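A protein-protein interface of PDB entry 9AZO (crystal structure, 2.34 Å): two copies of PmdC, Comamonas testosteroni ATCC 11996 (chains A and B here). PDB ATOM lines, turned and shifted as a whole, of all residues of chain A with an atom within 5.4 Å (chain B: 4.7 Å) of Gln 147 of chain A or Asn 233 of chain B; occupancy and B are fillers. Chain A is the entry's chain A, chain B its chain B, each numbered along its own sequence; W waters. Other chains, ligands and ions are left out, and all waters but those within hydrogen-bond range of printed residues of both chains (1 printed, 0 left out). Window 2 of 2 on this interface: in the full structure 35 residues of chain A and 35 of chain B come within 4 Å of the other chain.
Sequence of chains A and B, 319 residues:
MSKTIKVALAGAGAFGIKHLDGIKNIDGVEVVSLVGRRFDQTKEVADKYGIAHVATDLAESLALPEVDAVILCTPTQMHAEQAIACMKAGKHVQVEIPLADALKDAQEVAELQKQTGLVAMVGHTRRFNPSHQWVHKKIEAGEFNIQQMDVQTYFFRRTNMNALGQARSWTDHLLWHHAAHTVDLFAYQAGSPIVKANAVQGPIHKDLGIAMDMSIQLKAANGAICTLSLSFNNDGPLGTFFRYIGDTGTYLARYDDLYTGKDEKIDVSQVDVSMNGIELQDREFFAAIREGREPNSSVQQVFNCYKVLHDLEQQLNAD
Arg 158 of chain B touches Gln 147 of chain A (NH2 to OE1, 3.7 Å).
Asp 213 of chain B touches Gln 147 of chain A.
Gln 148 of chain A touches Ser 231 of chain B.
Asp 213 of chain B touches Ile 225 of chain A (C to CD1, 3.8 Å).
Ile 245 of chain A touches Ser 231 of chain B (CG2 to OG, 3.98 Å).
Ile 245 of chain A touches Asn 233 of chain B (CG2 to O, 3.4 Å).
CD1 of Ile 245 of chain A touches OD1 of Asn 234 of chain B, at 3.8 Å.
Thr 250 of chain A touches Asn 234 of chain B (CG2 to OD1, 3.96 Å).
Water W1 lies within hydrogen-bond range of the backbone carbonyl oxygen (O) of Asn 233 of chain B, the backbone carbonyl oxygen (O) of Gly 246 of chain A and the side-chain hydroxyl (OG1) of Thr 250 of chain A.
The side-chain amide nitrogen (NE2) of Gln 148 of chain A sits at hydrogen-bond distance from the side-chain carboxylate (OD1) of Asp 213 of chain B, 2.7 Å away.
The side-chain hydroxyl of Thr 250 of chain A is in hydrogen-bond range of the backbone NH of Asp 235 of chain B (3.2 Å).
The backbone carbonyl oxygen (O) of Gly 246 of chain A sits at hydrogen-bond distance from the guanidinium group (NH2) of Arg 158 of chain B, at 3.1 Å.
The side-chain amide nitrogen of Asn 233 of chain B sits close to the side-chain amide oxygen of Gln 147 of chain A, at 3.4 Å.
The backbone carbonyl oxygen of Asp 247 of chain A sits at hydrogen-bond distance from the guanidinium group of Arg 158 of chain B, 3.0 Å away.
Of the 10 printed residues of chain B, 6 touch a printed residue of chain A.
Of the 12 printed residues of chain A, 7 touch a printed residue of chain B.
Printed residues of chain A that touch a printed residue of chain B: Gln 147, Gln 148, Ile 225, Ile 245, Gly 246, Asp 247 and Thr 250.
Along chain A the printed residues that touch a printed residue of chain B span positions 147 to 250.
Among the printed residues, no Asp or Glu carboxylate lies within 4 Å of a Lys or Arg side-chain nitrogen of the other chain.
The backbone carbonyl oxygen (O) of Gln 148 of chain A is in hydrogen-bond range of the backbone NH (N) of Ile 245 of chain A, at 2.8 Å.
The backbone NH of Asn 234 of chain B sits at hydrogen-bond distance from the backbone carbonyl oxygen of Phe 155 of chain B, at 3.0 Å.
The side-chain carboxylate of Asp 213 of chain B sits at hydrogen-bond distance from the side-chain hydroxyl of Ser 231 of chain B (3.0 Å).
The backbone NH (N) of Asn 233 of chain B sits at hydrogen-bond distance from the side-chain hydroxyl (OG) of Ser 231 of chain B (2.7 Å).
The side-chain amide oxygen of Gln 147 of chain A lies close to the backbone carbonyl oxygen of Gly 246 of chain A, at 3.0 Å.
N of Ile 225 of chain A lies within hydrogen-bond range of O of Gln 147 of chain A, 3.0 Å away.
Gln 147 of chain A touches just these residues of chain B: Arg 158, Asp 213 and Asn 233.
Asn 233 of chain B touches just these residues of chain A: Gln 147 (3.1 Å) and Ile 245 (3.4 Å).
Of the printed residues of chain B, Asp 247 of chain A touches Arg 158 (3.0 Å).
Printed residues of chain B within 4 Å of Gly 246 of chain A: Arg 158.
Printed residues of chain A within 4 Å of Arg 158 of chain B: Gln 147, Gly 246 and Asp 247.
Of the printed residues of chain A, Asn 234 of chain B touches Ile 245 (3.8 Å) and Thr 250 (3.96 Å).
Of the printed residues of chain B, Ile 245 of chain A touches Ser 231, Asn 233 and Asn 234.
The nearest printed residue of chain B that does not touch Asp 247 of chain A is Asn 233 of chain B (5.9 Å).
No position is printed for both chains.
Of the 13 pairs that touch across the chains among the printed residues, none has its exchanged pair printed and touching as well.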
ATOM      1  N   ASN A 145      -3.003  -8.340  -5.694  1.00  0.00           N
ATOM      2  CA  ASN A 145      -1.926  -8.306  -6.688  1.00  0.00           C
ATOM      3  C   ASN A 145      -1.648  -6.884  -7.176  1.00  0.00           C
ATOM      4  O   ASN A 145      -2.563  -6.201  -7.643  1.00  0.00           O
ATOM      5  CB  ASN A 145      -2.298  -9.190  -7.869  1.00  0.00           C
ATOM      6  CG  ASN A 145      -2.473 -10.644  -7.464  1.00  0.00           C
ATOM      7  OD1 ASN A 145      -1.512 -11.403  -7.322  1.00  0.00           O
ATOM      8  ND2 ASN A 145      -3.724 -11.036  -7.274  1.00  0.00           N
ATOM      9  N   ILE A 146      -0.372  -6.483  -7.145  1.00  0.00           N
ATOM     10  CA  ILE A 146       0.083  -5.169  -7.621  1.00  0.00           C
ATOM     11  C   ILE A 146      -0.004  -5.046  -9.142  1.00  0.00           C
ATOM     12  O   ILE A 146       0.662  -5.793  -9.875  1.00  0.00           O
ATOM     13  CB  ILE A 146       1.529  -4.924  -7.175  1.00  0.00           C
ATOM     14  CG1 ILE A 146       1.614  -4.854  -5.647  1.00  0.00           C
ATOM     15  CG2 ILE A 146       2.152  -3.705  -7.926  1.00  0.00           C
ATOM     16  CD1 ILE A 146       3.033  -4.808  -5.146  1.00  0.00           C
ATOM     17  N   GLN A 147      -0.728  -4.022  -9.624  1.00  0.00           N
ATOM     18  CA  GLN A 147      -0.685  -3.605 -11.023  1.00  0.00           C
ATOM     19  C   GLN A 147       0.345  -2.489 -11.255  1.00  0.00           C
ATOM     20  O   GLN A 147       1.134  -2.562 -12.205  1.00  0.00           O
ATOM     21  CB  GLN A 147      -2.097  -3.163 -11.457  1.00  0.00           C
ATOM     22  CG  GLN A 147      -3.205  -4.266 -11.421  1.00  0.00           C
ATOM     23  CD  GLN A 147      -4.647  -3.747 -11.075  1.00  0.00           C
ATOM     24  OE1 GLN A 147      -4.822  -2.707 -10.418  1.00  0.00           O
ATOM     25  NE2 GLN A 147      -5.670  -4.473 -11.537  1.00  0.00           N
ATOM     26  N   GLN A 148       0.386  -1.470 -10.389  1.00  0.00           N
ATOM     27  CA  GLN A 148       1.368  -0.399 -10.534  1.00  0.00           C
ATOM     28  C   GLN A 148       1.819   0.117  -9.166  1.00  0.00           C
ATOM     29  O   GLN A 148       0.986   0.369  -8.296  1.00  0.00           O
ATOM     30  CB  GLN A 148       0.782   0.726 -11.385  1.00  0.00           C
ATOM     31  CG  GLN A 148       1.665   1.936 -11.556  1.00  0.00           C
ATOM     32  CD  GLN A 148       1.076   2.892 -12.593  1.00  0.00           C
ATOM     33  OE1 GLN A 148       1.785   3.737 -13.112  1.00  0.00           O
ATOM     34  NE2 GLN A 148      -0.222   2.751 -12.900  1.00  0.00           N
ATOM     35  N   MET A 149       3.114   0.370  -9.013  1.00  0.00           N
ATOM     36  CA  MET A 149       3.652   1.126  -7.876  1.00  0.00           C
ATOM     37  C   MET A 149       4.152   2.491  -8.322  1.00  0.00           C
ATOM     38  O   MET A 149       5.027   2.557  -9.192  1.00  0.00           O
ATOM     39  CB  MET A 149       4.820   0.420  -7.183  1.00  0.00           C
ATOM     40  CG  MET A 149       4.459  -0.624  -6.156  1.00  0.00           C
ATOM     41  SD  MET A 149       5.975  -1.459  -5.640  1.00  0.00           S
ATOM     42  CE  MET A 149       6.898  -0.101  -4.887  1.00  0.00           C
ATOM     43  N   GLY A 223       3.911  -8.429 -15.686  1.00  0.00           N
ATOM     44  CA  GLY A 223       3.232  -7.278 -16.232  1.00  0.00           C
ATOM     45  C   GLY A 223       3.036  -6.105 -15.279  1.00  0.00           C
ATOM     46  O   GLY A 223       2.655  -5.024 -15.742  1.00  0.00           O
ATOM     47  N   ALA A 224       3.250  -6.274 -13.974  1.00  0.00           N
ATOM     48  CA  ALA A 224       3.208  -5.113 -13.078  1.00  0.00           C
ATOM     49  C   ALA A 224       4.226  -4.052 -13.507  1.00  0.00           C
ATOM     50  O   ALA A 224       5.289  -4.377 -14.033  1.00  0.00           O
ATOM     51  CB  ALA A 224       3.482  -5.539 -11.636  1.00  0.00           C
ATOM     52  N   ILE A 225       3.886  -2.764 -13.317  1.00  0.00           N
ATOM     53  CA  ILE A 225       4.812  -1.678 -13.650  1.00  0.00           C
ATOM     54  C   ILE A 225       5.035  -0.846 -12.387  1.00  0.00           C
ATOM     55  O   ILE A 225       4.211  -0.808 -11.476  1.00  0.00           O
ATOM     56  CB  ILE A 225       4.388  -0.756 -14.813  1.00  0.00           C
ATOM     57  CG1 ILE A 225       3.073  -0.038 -14.538  1.00  0.00           C
ATOM     58  CG2 ILE A 225       4.258  -1.538 -16.111  1.00  0.00           C
ATOM     59  CD1 ILE A 225       2.821   1.068 -15.565  1.00  0.00           C
ATOM     60  N   ILE A 245      -1.090   0.368  -6.353  1.00  0.00           N
ATOM     61  CA  ILE A 245      -2.393   0.254  -7.016  1.00  0.00           C
ATOM     62  C   ILE A 245      -2.583  -1.199  -7.441  1.00  0.00           C
ATOM     63  O   ILE A 245      -1.786  -1.716  -8.225  1.00  0.00           O
ATOM     64  CB  ILE A 245      -2.526   1.192  -8.222  1.00  0.00           C
ATOM     65  CG1 ILE A 245      -2.178   2.635  -7.865  1.00  0.00           C
ATOM     66  CG2 ILE A 245      -3.850   1.012  -8.893  1.00  0.00           C
ATOM     67  CD1 ILE A 245      -2.180   3.553  -9.066  1.00  0.00           C
ATOM     68  N   GLY A 246      -3.505  -1.913  -6.800  1.00  0.00           N
ATOM     69  CA  GLY A 246      -3.769  -3.302  -7.131  1.00  0.00           C
ATOM     70  C   GLY A 246      -5.160  -3.650  -7.616  1.00  0.00           C
ATOM     71  O   GLY A 246      -6.051  -2.799  -7.680  1.00  0.00           O
ATOM     72  N   ASP A 247      -5.410  -4.951  -7.750  1.00  0.00           N
ATOM     73  CA  ASP A 247      -6.719  -5.429  -8.180  1.00  0.00           C
ATOM     74  C   ASP A 247      -7.775  -5.263  -7.099  1.00  0.00           C
ATOM     75  O   ASP A 247      -8.939  -4.980  -7.408  1.00  0.00           O
ATOM     76  CB  ASP A 247      -6.629  -6.882  -8.681  1.00  0.00           C
ATOM     77  CG  ASP A 247      -6.036  -7.845  -7.652  1.00  0.00           C
ATOM     78  OD1 ASP A 247      -5.521  -7.395  -6.601  1.00  0.00           O
ATOM     79  OD2 ASP A 247      -6.090  -9.073  -7.894  1.00  0.00           O
ATOM     80  N   THR A 250      -6.027  -0.013  -3.121  1.00  0.00           N
ATOM     81  CA  THR A 250      -4.936   0.941  -3.222  1.00  0.00           C
ATOM     82  C   THR A 250      -4.422   1.263  -1.830  1.00  0.00           C
ATOM     83  O   THR A 250      -5.203   1.488  -0.899  1.00  0.00           O
ATOM     84  CB  THR A 250      -5.419   2.209  -3.926  1.00  0.00           C
ATOM     85  OG1 THR A 250      -5.790   1.887  -5.266  1.00  0.00           O
ATOM     86  CG2 THR A 250      -4.364   3.292  -3.928  1.00  0.00           C
ATOM     87  N   PHE B 155      -7.689   7.398 -12.354  1.00  0.00           N
ATOM     88  CA  PHE B 155      -9.135   7.219 -12.274  1.00  0.00           C
ATOM     89  C   PHE B 155      -9.351   5.820 -11.729  1.00  0.00           C
ATOM     90  O   PHE B 155      -8.417   5.012 -11.675  1.00  0.00           O
ATOM     91  CB  PHE B 155      -9.837   7.395 -13.623  1.00  0.00           C
ATOM     92  CG  PHE B 155      -9.620   8.729 -14.203  1.00  0.00           C
ATOM     93  CD1 PHE B 155     -10.402   9.802 -13.789  1.00  0.00           C
ATOM     94  CD2 PHE B 155      -8.532   8.954 -15.058  1.00  0.00           C
ATOM     95  CE1 PHE B 155     -10.175  11.059 -14.291  1.00  0.00           C
ATOM     96  CE2 PHE B 155      -8.285  10.211 -15.555  1.00  0.00           C
ATOM     97  CZ  PHE B 155      -9.109  11.274 -15.169  1.00  0.00           C
ATOM     98  N   PHE B 156     -10.553   5.564 -11.237  1.00  0.00           N
ATOM     99  CA  PHE B 156     -10.972   4.207 -10.941  1.00  0.00           C
ATOM    100  C   PHE B 156     -11.980   3.955 -12.049  1.00  0.00           C
ATOM    101  O   PHE B 156     -13.169   4.261 -11.907  1.00  0.00           O
ATOM    102  CB  PHE B 156     -11.527   4.151  -9.523  1.00  0.00           C
ATOM    103  CG  PHE B 156     -11.668   2.777  -8.973  1.00  0.00           C
ATOM    104  CD1 PHE B 156     -10.559   1.941  -8.929  1.00  0.00           C
ATOM    105  CD2 PHE B 156     -12.840   2.353  -8.386  1.00  0.00           C
ATOM    106  CE1 PHE B 156     -10.640   0.674  -8.384  1.00  0.00           C
ATOM    107  CE2 PHE B 156     -12.927   1.088  -7.824  1.00  0.00           C
ATOM    108  CZ  PHE B 156     -11.824   0.254  -7.822  1.00  0.00           C
ATOM    109  N   ARG B 158     -12.793   0.854 -14.398  1.00  0.00           N
ATOM    110  CA  ARG B 158     -12.821  -0.506 -14.924  1.00  0.00           C
ATOM    111  C   ARG B 158     -13.998  -0.738 -15.863  1.00  0.00           C
ATOM    112  O   ARG B 158     -14.191  -1.861 -16.322  1.00  0.00           O
ATOM    113  CB  ARG B 158     -12.833  -1.495 -13.746  1.00  0.00           C
ATOM    114  CG  ARG B 158     -11.546  -1.407 -12.961  1.00  0.00           C
ATOM    115  CD  ARG B 158     -11.441  -2.326 -11.770  1.00  0.00           C
ATOM    116  NE  ARG B 158     -10.094  -2.153 -11.229  1.00  0.00           N
ATOM    117  CZ  ARG B 158      -9.694  -2.474 -10.003  1.00  0.00           C
ATOM    118  NH1 ARG B 158     -10.506  -3.050  -9.130  1.00  0.00           N
ATOM    119  NH2 ARG B 158      -8.414  -2.304  -9.682  1.00  0.00           N
ATOM    120  N   MET B 212      -4.598  -0.574 -18.778  1.00  0.00           N
ATOM    121  CA  MET B 212      -5.114   0.015 -17.531  1.00  0.00           C
ATOM    122  C   MET B 212      -4.058   0.793 -16.721  1.00  0.00           C
ATOM    123  O   MET B 212      -4.431   1.527 -15.797  1.00  0.00           O
ATOM    124  CB  MET B 212      -5.763  -1.077 -16.665  1.00  0.00           C
ATOM    125  CG  MET B 212      -6.948  -1.761 -17.370  1.00  0.00           C
ATOM    126  SD  MET B 212      -8.389  -0.847 -18.011  1.00  0.00           S
ATOM    127  CE  MET B 212      -9.239  -0.384 -16.484  1.00  0.00           C
ATOM    128  N   ASP B 213      -2.759   0.619 -17.009  1.00  0.00           N
ATOM    129  CA  ASP B 213      -1.650   1.279 -16.317  1.00  0.00           C
ATOM    130  C   ASP B 213      -0.555   1.641 -17.302  1.00  0.00           C
ATOM    131  O   ASP B 213      -0.227   0.851 -18.184  1.00  0.00           O
ATOM    132  CB  ASP B 213      -0.978   0.454 -15.206  1.00  0.00           C
ATOM    133  CG  ASP B 213      -1.895   0.092 -14.102  1.00  0.00           C
ATOM    134  OD1 ASP B 213      -2.201   1.006 -13.290  1.00  0.00           O
ATOM    135  OD2 ASP B 213      -2.306  -1.086 -14.031  1.00  0.00           O
ATOM    136  N   SER B 231      -3.224   5.685 -14.597  1.00  0.00           N
ATOM    137  CA  SER B 231      -3.990   4.506 -14.184  1.00  0.00           C
ATOM    138  C   SER B 231      -5.493   4.654 -14.294  1.00  0.00           C
ATOM    139  O   SER B 231      -6.046   5.720 -14.009  1.00  0.00           O
ATOM    140  CB  SER B 231      -3.700   4.114 -12.725  1.00  0.00           C
ATOM    141  OG  SER B 231      -4.381   2.907 -12.355  1.00  0.00           O
ATOM    142  N   PHE B 232      -6.139   3.606 -14.788  1.00  0.00           N
ATOM    143  CA  PHE B 232      -7.583   3.406 -14.634  1.00  0.00           C
ATOM    144  C   PHE B 232      -7.925   2.460 -13.483  1.00  0.00           C
ATOM    145  O   PHE B 232      -9.104   2.217 -13.223  1.00  0.00           O
ATOM    146  CB  PHE B 232      -8.142   2.835 -15.943  1.00  0.00           C
ATOM    147  CG  PHE B 232      -8.280   3.837 -17.066  1.00  0.00           C
ATOM    148  CD1 PHE B 232      -8.308   5.194 -16.821  1.00  0.00           C
ATOM    149  CD2 PHE B 232      -8.220   3.407 -18.391  1.00  0.00           C
ATOM    150  CE1 PHE B 232      -8.443   6.102 -17.858  1.00  0.00           C
ATOM    151  CE2 PHE B 232      -8.297   4.322 -19.457  1.00  0.00           C
ATOM    152  CZ  PHE B 232      -8.418   5.663 -19.192  1.00  0.00           C
ATOM    153  N   ASN B 233      -6.915   1.962 -12.765  1.00  0.00           N
ATOM    154  CA  ASN B 233      -7.045   1.083 -11.600  1.00  0.00           C
ATOM    155  C   ASN B 233      -6.986   1.776 -10.217  1.00  0.00           C
ATOM    156  O   ASN B 233      -7.196   1.105  -9.201  1.00  0.00           O
ATOM    157  CB  ASN B 233      -5.892   0.058 -11.672  1.00  0.00           C
ATOM    158  CG  ASN B 233      -6.165  -1.067 -12.665  1.00  0.00           C
ATOM    159  OD1 ASN B 233      -7.235  -1.641 -12.700  1.00  0.00           O
ATOM    160  ND2 ASN B 233      -5.173  -1.366 -13.493  1.00  0.00           N
ATOM    161  N   ASN B 234      -6.776   3.088 -10.154  1.00  0.00           N
ATOM    162  CA  ASN B 234      -6.560   3.839  -8.907  1.00  0.00           C
ATOM    163  C   ASN B 234      -7.871   4.043  -8.142  1.00  0.00           C
ATOM    164  O   ASN B 234      -8.724   4.848  -8.524  1.00  0.00           O
ATOM    165  CB  ASN B 234      -5.826   5.137  -9.154  1.00  0.00           C
ATOM    166  CG  ASN B 234      -5.633   5.896  -7.876  1.00  0.00           C
ATOM    167  OD1 ASN B 234      -4.708   5.583  -7.143  1.00  0.00           O
ATOM    168  ND2 ASN B 234      -6.482   6.867  -7.592  1.00  0.00           N
ATOM    169  N   ASP B 235      -8.049   3.282  -7.063  1.00  0.00           N
ATOM    170  CA  ASP B 235      -9.142   3.524  -6.125  1.00  0.00           C
ATOM    171  C   ASP B 235      -8.921   4.639  -5.099  1.00  0.00           C
ATOM    172  O   ASP B 235      -8.594   4.419  -3.936  1.00  0.00           O
ATOM    173  CB  ASP B 235      -9.494   2.233  -5.400  1.00  0.00           C
ATOM    174  CG  ASP B 235     -10.780   2.351  -4.593  1.00  0.00           C
ATOM    175  OD1 ASP B 235     -11.566   3.303  -4.813  1.00  0.00           O
ATOM    176  OD2 ASP B 235     -11.026   1.465  -3.757  1.00  0.00           O
HETATM  177  O   HOH W   1      -7.019  -0.294  -6.867  1.00  0.00           O
